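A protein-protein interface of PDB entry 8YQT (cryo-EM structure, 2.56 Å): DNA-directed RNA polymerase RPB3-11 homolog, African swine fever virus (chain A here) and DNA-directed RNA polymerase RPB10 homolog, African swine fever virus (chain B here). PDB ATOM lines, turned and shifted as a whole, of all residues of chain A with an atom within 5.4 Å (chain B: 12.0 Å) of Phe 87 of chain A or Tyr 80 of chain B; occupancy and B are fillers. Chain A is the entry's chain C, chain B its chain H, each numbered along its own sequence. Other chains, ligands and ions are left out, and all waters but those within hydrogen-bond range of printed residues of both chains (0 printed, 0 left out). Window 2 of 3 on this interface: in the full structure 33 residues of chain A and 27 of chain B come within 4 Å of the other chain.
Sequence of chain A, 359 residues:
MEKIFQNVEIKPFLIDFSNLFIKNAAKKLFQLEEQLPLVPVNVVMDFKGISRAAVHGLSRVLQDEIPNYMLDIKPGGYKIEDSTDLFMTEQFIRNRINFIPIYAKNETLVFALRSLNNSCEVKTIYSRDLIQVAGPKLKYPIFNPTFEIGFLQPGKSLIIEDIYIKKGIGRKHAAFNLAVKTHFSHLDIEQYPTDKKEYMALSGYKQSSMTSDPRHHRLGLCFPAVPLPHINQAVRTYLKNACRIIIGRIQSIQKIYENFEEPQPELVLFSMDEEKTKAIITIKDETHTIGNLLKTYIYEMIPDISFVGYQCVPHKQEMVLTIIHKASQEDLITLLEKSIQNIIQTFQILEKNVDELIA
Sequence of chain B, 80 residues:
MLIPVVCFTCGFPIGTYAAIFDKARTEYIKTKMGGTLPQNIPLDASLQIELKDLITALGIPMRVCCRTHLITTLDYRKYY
OD2 of Asp 85 of chain A is in hydrogen-bond range of N of Phe 87 of chain A, 3.1 Å away.
The side-chain carboxylate of Asp 85 of chain A sits at hydrogen-bond distance from the backbone NH of Gln 153 of chain A, 3.1 Å away.
The side-chain sulfur (SD) of Met 88 of chain A is in hydrogen-bond range of the backbone NH (N) of Phe 151 of chain A.
The backbone NH (N) of Phe 92 of chain A sits at hydrogen-bond distance from the side-chain hydroxyl (OG1) of Thr 89 of chain A, at 3.5 Å.
The backbone carbonyl oxygen of Met 1 of chain B sits at hydrogen-bond distance from the backbone NH of Tyr 76 of chain B, 2.8 Å away.
OD2 of Asp 75 of chain B is in salt-bridge range of NH2 of Arg 77 of chain B, 3.2 Å away.
Of the 8 printed residues of chain A, 4 touch a printed residue of chain B.
Hydrophobic or aromatic side chains of chain A within 4 Å of the printed part of chain B: Phe 87, Phe 92 and Phe 151.
Among the printed residues, no Asp or Glu carboxylate lies within 4 Å of a Lys or Arg side-chain nitrogen of the other chain.
Phe 87 of chain A touches Met 1 of chain B.
CE1 of Phe 87 of chain A touches OH of Tyr 76 of chain B (3.5 Å).
CZ of Phe 87 of chain A touches CZ of Tyr 80 of chain B, 3.5 Å away.
CZ of Phe 92 of chain A touches CB of Met 1 of chain B (3.8 Å).
Leu 2 of chain B touches Phe 151 of chain A (CD2 to CD2, 3.6 Å).
CB of Tyr 76 of chain B touches CZ of Phe 151 of chain A, 3.8 Å away.
Phe 151 of chain A touches Arg 77 of chain B.
Gln 153 of chain A touches Tyr 80 of chain B (OE1 to CE2, 3.9 Å).
Of chain B, only Met 1 (3.5 Å), Tyr 76 (3.5 Å) and Tyr 80 (3.5 Å) come within 4 Å of Phe 87 of chain A.
No residue of chain B comes within 4 Å of Leu 86 of chain A.
Of the printed residues of chain A, Met 1 of chain B touches Phe 87 and Phe 92.
Printed residues of chain A within 4 Å of Arg 77 of chain B: Phe 151.
Of the printed residues of chain A, Tyr 76 of chain B touches Phe 87 (3.5 Å) and Phe 151 (3.8 Å).
Leu 74 of chain B touches none of the printed residues of chain A.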
ATOM      1  N   ASP A  85     -19.767  15.410  17.837  1.00  0.00           N
ATOM      2  CA  ASP A  85     -18.543  16.194  17.788  1.00  0.00           C
ATOM      3  C   ASP A  85     -18.517  17.046  16.530  1.00  0.00           C
ATOM      4  O   ASP A  85     -18.747  16.549  15.423  1.00  0.00           O
ATOM      5  CB  ASP A  85     -17.309  15.300  17.835  1.00  0.00           C
ATOM      6  CG  ASP A  85     -16.034  16.094  18.057  1.00  0.00           C
ATOM      7  OD1 ASP A  85     -15.760  16.474  19.212  1.00  0.00           O
ATOM      8  OD2 ASP A  85     -15.314  16.355  17.073  1.00  0.00           O
ATOM      9  N   LEU A  86     -18.224  18.328  16.704  1.00  0.00           N
ATOM     10  CA  LEU A  86     -18.272  19.283  15.611  1.00  0.00           C
ATOM     11  C   LEU A  86     -16.976  19.360  14.818  1.00  0.00           C
ATOM     12  O   LEU A  86     -16.975  19.917  13.716  1.00  0.00           O
ATOM     13  CB  LEU A  86     -18.616  20.668  16.159  1.00  0.00           C
ATOM     14  CG  LEU A  86     -19.936  20.815  16.915  1.00  0.00           C
ATOM     15  CD1 LEU A  86     -20.104  22.241  17.396  1.00  0.00           C
ATOM     16  CD2 LEU A  86     -21.108  20.395  16.051  1.00  0.00           C
ATOM     17  N   PHE A  87     -15.880  18.813  15.338  1.00  0.00           N
ATOM     18  CA  PHE A  87     -14.587  18.909  14.675  1.00  0.00           C
ATOM     19  C   PHE A  87     -14.178  17.631  13.962  1.00  0.00           C
ATOM     20  O   PHE A  87     -13.475  17.700  12.951  1.00  0.00           O
ATOM     21  CB  PHE A  87     -13.501  19.291  15.687  1.00  0.00           C
ATOM     22  CG  PHE A  87     -13.667  20.668  16.255  1.00  0.00           C
ATOM     23  CD1 PHE A  87     -13.138  21.766  15.608  1.00  0.00           C
ATOM     24  CD2 PHE A  87     -14.363  20.865  17.434  1.00  0.00           C
ATOM     25  CE1 PHE A  87     -13.292  23.030  16.126  1.00  0.00           C
ATOM     26  CE2 PHE A  87     -14.521  22.128  17.954  1.00  0.00           C
ATOM     27  CZ  PHE A  87     -13.984  23.210  17.299  1.00  0.00           C
ATOM     28  N   MET A  88     -14.598  16.469  14.457  1.00  0.00           N
ATOM     29  CA  MET A  88     -14.296  15.195  13.809  1.00  0.00           C
ATOM     30  C   MET A  88     -15.321  14.970  12.707  1.00  0.00           C
ATOM     31  O   MET A  88     -16.327  14.288  12.892  1.00  0.00           O
ATOM     32  CB  MET A  88     -14.296  14.058  14.823  1.00  0.00           C
ATOM     33  CG  MET A  88     -13.164  14.135  15.828  1.00  0.00           C
ATOM     34  SD  MET A  88     -11.542  14.288  15.057  1.00  0.00           S
ATOM     35  CE  MET A  88     -11.114  15.970  15.473  1.00  0.00           C
ATOM     36  N   THR A  89     -15.060  15.557  11.545  1.00  0.00           N
ATOM     37  CA  THR A  89     -15.930  15.380  10.398  1.00  0.00           C
ATOM     38  C   THR A  89     -15.694  14.013   9.764  1.00  0.00           C
ATOM     39  O   THR A  89     -14.697  13.339  10.026  1.00  0.00           O
ATOM     40  CB  THR A  89     -15.702  16.494   9.377  1.00  0.00           C
ATOM     41  OG1 THR A  89     -14.366  16.417   8.876  1.00  0.00           O
ATOM     42  CG2 THR A  89     -15.910  17.849  10.024  1.00  0.00           C
ATOM     43  N   PHE A  92     -12.446  13.829   7.539  1.00  0.00           N
ATOM     44  CA  PHE A  92     -11.220  13.703   8.318  1.00  0.00           C
ATOM     45  C   PHE A  92     -11.045  12.287   8.854  1.00  0.00           C
ATOM     46  O   PHE A  92      -9.999  11.659   8.657  1.00  0.00           O
ATOM     47  CB  PHE A  92     -11.243  14.720   9.461  1.00  0.00           C
ATOM     48  CG  PHE A  92      -9.973  14.776  10.257  1.00  0.00           C
ATOM     49  CD1 PHE A  92      -8.853  15.411   9.755  1.00  0.00           C
ATOM     50  CD2 PHE A  92      -9.905  14.200  11.512  1.00  0.00           C
ATOM     51  CE1 PHE A  92      -7.691  15.462  10.484  1.00  0.00           C
ATOM     52  CE2 PHE A  92      -8.743  14.251  12.246  1.00  0.00           C
ATOM     53  CZ  PHE A  92      -7.636  14.884  11.731  1.00  0.00           C
ATOM     54  N   PHE A 151     -10.053  13.044  18.205  1.00  0.00           N
ATOM     55  CA  PHE A 151     -10.239  13.565  19.551  1.00  0.00           C
ATOM     56  C   PHE A 151     -11.608  14.219  19.656  1.00  0.00           C
ATOM     57  O   PHE A 151     -12.091  14.827  18.701  1.00  0.00           O
ATOM     58  CB  PHE A 151      -9.140  14.562  19.944  1.00  0.00           C
ATOM     59  CG  PHE A 151      -8.928  15.669  18.954  1.00  0.00           C
ATOM     60  CD1 PHE A 151      -9.585  16.877  19.094  1.00  0.00           C
ATOM     61  CD2 PHE A 151      -8.050  15.513  17.899  1.00  0.00           C
ATOM     62  CE1 PHE A 151      -9.384  17.896  18.194  1.00  0.00           C
ATOM     63  CE2 PHE A 151      -7.846  16.530  16.997  1.00  0.00           C
ATOM     64  CZ  PHE A 151      -8.513  17.722  17.145  1.00  0.00           C
ATOM     65  N   GLN A 153     -14.194  16.770  21.918  1.00  0.00           N
ATOM     66  CA  GLN A 153     -14.355  17.822  22.900  1.00  0.00           C
ATOM     67  C   GLN A 153     -15.199  17.310  24.064  1.00  0.00           C
ATOM     68  O   GLN A 153     -15.914  16.317  23.927  1.00  0.00           O
ATOM     69  CB  GLN A 153     -15.011  19.040  22.258  1.00  0.00           C
ATOM     70  CG  GLN A 153     -14.275  19.568  21.044  1.00  0.00           C
ATOM     71  CD  GLN A 153     -12.868  20.010  21.366  1.00  0.00           C
ATOM     72  OE1 GLN A 153     -12.627  20.660  22.380  1.00  0.00           O
ATOM     73  NE2 GLN A 153     -11.926  19.654  20.507  1.00  0.00           N
ATOM     74  N   MET B   1      -5.058  18.081  11.575  1.00  0.00           N
ATOM     75  CA  MET B   1      -5.367  18.441  12.951  1.00  0.00           C
ATOM     76  C   MET B   1      -4.574  17.570  13.919  1.00  0.00           C
ATOM     77  O   MET B   1      -4.533  17.832  15.117  1.00  0.00           O
ATOM     78  CB  MET B   1      -6.868  18.307  13.211  1.00  0.00           C
ATOM     79  CG  MET B   1      -7.682  19.501  12.741  1.00  0.00           C
ATOM     80  SD  MET B   1      -9.373  19.497  13.358  1.00  0.00           S
ATOM     81  CE  MET B   1     -10.109  18.241  12.323  1.00  0.00           C
ATOM     82  N   LEU B   2      -3.945  16.530  13.380  1.00  0.00           N
ATOM     83  CA  LEU B   2      -3.120  15.611  14.146  1.00  0.00           C
ATOM     84  C   LEU B   2      -1.909  15.240  13.306  1.00  0.00           C
ATOM     85  O   LEU B   2      -1.822  15.578  12.126  1.00  0.00           O
ATOM     86  CB  LEU B   2      -3.893  14.348  14.539  1.00  0.00           C
ATOM     87  CG  LEU B   2      -5.087  14.475  15.480  1.00  0.00           C
ATOM     88  CD1 LEU B   2      -5.870  13.183  15.504  1.00  0.00           C
ATOM     89  CD2 LEU B   2      -4.619  14.832  16.870  1.00  0.00           C
ATOM     90  N   LEU B  74       1.347  20.273  13.089  1.00  0.00           N
ATOM     91  CA  LEU B  74       0.666  20.950  14.183  1.00  0.00           C
ATOM     92  C   LEU B  74      -0.451  20.082  14.742  1.00  0.00           C
ATOM     93  O   LEU B  74      -1.135  19.370  14.006  1.00  0.00           O
ATOM     94  CB  LEU B  74       0.091  22.280  13.709  1.00  0.00           C
ATOM     95  CG  LEU B  74       1.044  23.285  13.076  1.00  0.00           C
ATOM     96  CD1 LEU B  74       0.259  24.472  12.568  1.00  0.00           C
ATOM     97  CD2 LEU B  74       2.097  23.722  14.067  1.00  0.00           C
ATOM     98  N   ASP B  75      -0.637  20.153  16.053  1.00  0.00           N
ATOM     99  CA  ASP B  75      -1.692  19.420  16.736  1.00  0.00           C
ATOM    100  C   ASP B  75      -2.795  20.398  17.117  1.00  0.00           C
ATOM    101  O   ASP B  75      -2.554  21.353  17.859  1.00  0.00           O
ATOM    102  CB  ASP B  75      -1.141  18.706  17.969  1.00  0.00           C
ATOM    103  CG  ASP B  75      -2.131  17.744  18.576  1.00  0.00           C
ATOM    104  OD1 ASP B  75      -3.208  17.544  17.982  1.00  0.00           O
ATOM    105  OD2 ASP B  75      -1.832  17.177  19.644  1.00  0.00           O
ATOM    106  N   TYR B  76      -4.002  20.157  16.606  1.00  0.00           N
ATOM    107  CA  TYR B  76      -5.129  21.041  16.876  1.00  0.00           C
ATOM    108  C   TYR B  76      -5.515  21.056  18.347  1.00  0.00           C
ATOM    109  O   TYR B  76      -6.067  22.053  18.819  1.00  0.00           O
ATOM    110  CB  TYR B  76      -6.325  20.619  16.025  1.00  0.00           C
ATOM    111  CG  TYR B  76      -7.370  21.687  15.813  1.00  0.00           C
ATOM    112  CD1 TYR B  76      -7.270  22.582  14.762  1.00  0.00           C
ATOM    113  CD2 TYR B  76      -8.473  21.780  16.645  1.00  0.00           C
ATOM    114  CE1 TYR B  76      -8.227  23.548  14.558  1.00  0.00           C
ATOM    115  CE2 TYR B  76      -9.435  22.741  16.447  1.00  0.00           C
ATOM    116  CZ  TYR B  76      -9.306  23.622  15.403  1.00  0.00           C
ATOM    117  OH  TYR B  76     -10.264  24.582  15.204  1.00  0.00           O
ATOM    118  N   ARG B  77      -5.242  19.975  19.077  1.00  0.00           N
ATOM    119  CA  ARG B  77      -5.570  19.933  20.497  1.00  0.00           C
ATOM    120  C   ARG B  77      -4.755  20.939  21.297  1.00  0.00           C
ATOM    121  O   ARG B  77      -5.211  21.409  22.344  1.00  0.00           O
ATOM    122  CB  ARG B  77      -5.346  18.526  21.044  1.00  0.00           C
ATOM    123  CG  ARG B  77      -6.278  17.484  20.480  1.00  0.00           C
ATOM    124  CD  ARG B  77      -5.894  16.094  20.944  1.00  0.00           C
ATOM    125  NE  ARG B  77      -4.663  15.634  20.317  1.00  0.00           N
ATOM    126  CZ  ARG B  77      -4.086  14.466  20.563  1.00  0.00           C
ATOM    127  NH1 ARG B  77      -4.612  13.602  21.414  1.00  0.00           N
ATOM    128  NH2 ARG B  77      -2.955  14.158  19.939  1.00  0.00           N
ATOM    129  N   LYS B  78      -3.558  21.277  20.829  1.00  0.00           N
ATOM    130  CA  LYS B  78      -2.666  22.178  21.541  1.00  0.00           C
ATOM    131  C   LYS B  78      -2.955  23.647  21.270  1.00  0.00           C
ATOM    132  O   LYS B  78      -2.386  24.508  21.946  1.00  0.00           O
ATOM    133  CB  LYS B  78      -1.214  21.870  21.174  1.00  0.00           C
ATOM    134  CG  LYS B  78      -0.912  20.395  21.071  1.00  0.00           C
ATOM    135  CD  LYS B  78      -0.303  19.863  22.345  1.00  0.00           C
ATOM    136  CE  LYS B  78       0.545  18.642  22.064  1.00  0.00           C
ATOM    137  NZ  LYS B  78       1.522  18.902  20.975  1.00  0.00           N
ATOM    138  N   TYR B  79      -3.817  23.957  20.304  1.00  0.00           N
ATOM    139  CA  TYR B  79      -4.156  25.332  19.982  1.00  0.00           C
ATOM    140  C   TYR B  79      -5.606  25.685  20.254  1.00  0.00           C
ATOM    141  O   TYR B  79      -5.941  26.873  20.253  1.00  0.00           O
ATOM    142  CB  TYR B  79      -3.851  25.629  18.506  1.00  0.00           C
ATOM    143  CG  TYR B  79      -2.390  25.528  18.157  1.00  0.00           C
ATOM    144  CD1 TYR B  79      -1.517  26.560  18.450  1.00  0.00           C
ATOM    145  CD2 TYR B  79      -1.884  24.397  17.541  1.00  0.00           C
ATOM    146  CE1 TYR B  79      -0.181  26.469  18.137  1.00  0.00           C
ATOM    147  CE2 TYR B  79      -0.551  24.297  17.225  1.00  0.00           C
ATOM    148  CZ  TYR B  79       0.296  25.338  17.523  1.00  0.00           C
ATOM    149  OH  TYR B  79       1.632  25.244  17.207  1.00  0.00           O
ATOM    150  N   TYR B  80      -6.468  24.703  20.482  1.00  0.00           N
ATOM    151  CA  TYR B  80      -7.878  24.956  20.727  1.00  0.00           C
ATOM    152  C   TYR B  80      -8.283  24.455  22.106  1.00  0.00           C
ATOM    153  O   TYR B  80      -8.317  23.251  22.350  1.00  0.00           O
ATOM    154  CB  TYR B  80      -8.732  24.293  19.651  1.00  0.00           C
ATOM    155  CG  TYR B  80     -10.200  24.626  19.742  1.00  0.00           C
ATOM    156  CD1 TYR B  80     -10.680  25.852  19.314  1.00  0.00           C
ATOM    157  CD2 TYR B  80     -11.105  23.715  20.258  1.00  0.00           C
ATOM    158  CE1 TYR B  80     -12.018  26.158  19.399  1.00  0.00           C
ATOM    159  CE2 TYR B  80     -12.443  24.014  20.346  1.00  0.00           C
ATOM    160  CZ  TYR B  80     -12.893  25.237  19.914  1.00  0.00           C
ATOM    161  OH  TYR B  80     -14.229  25.544  19.998  1.00  0.00           O
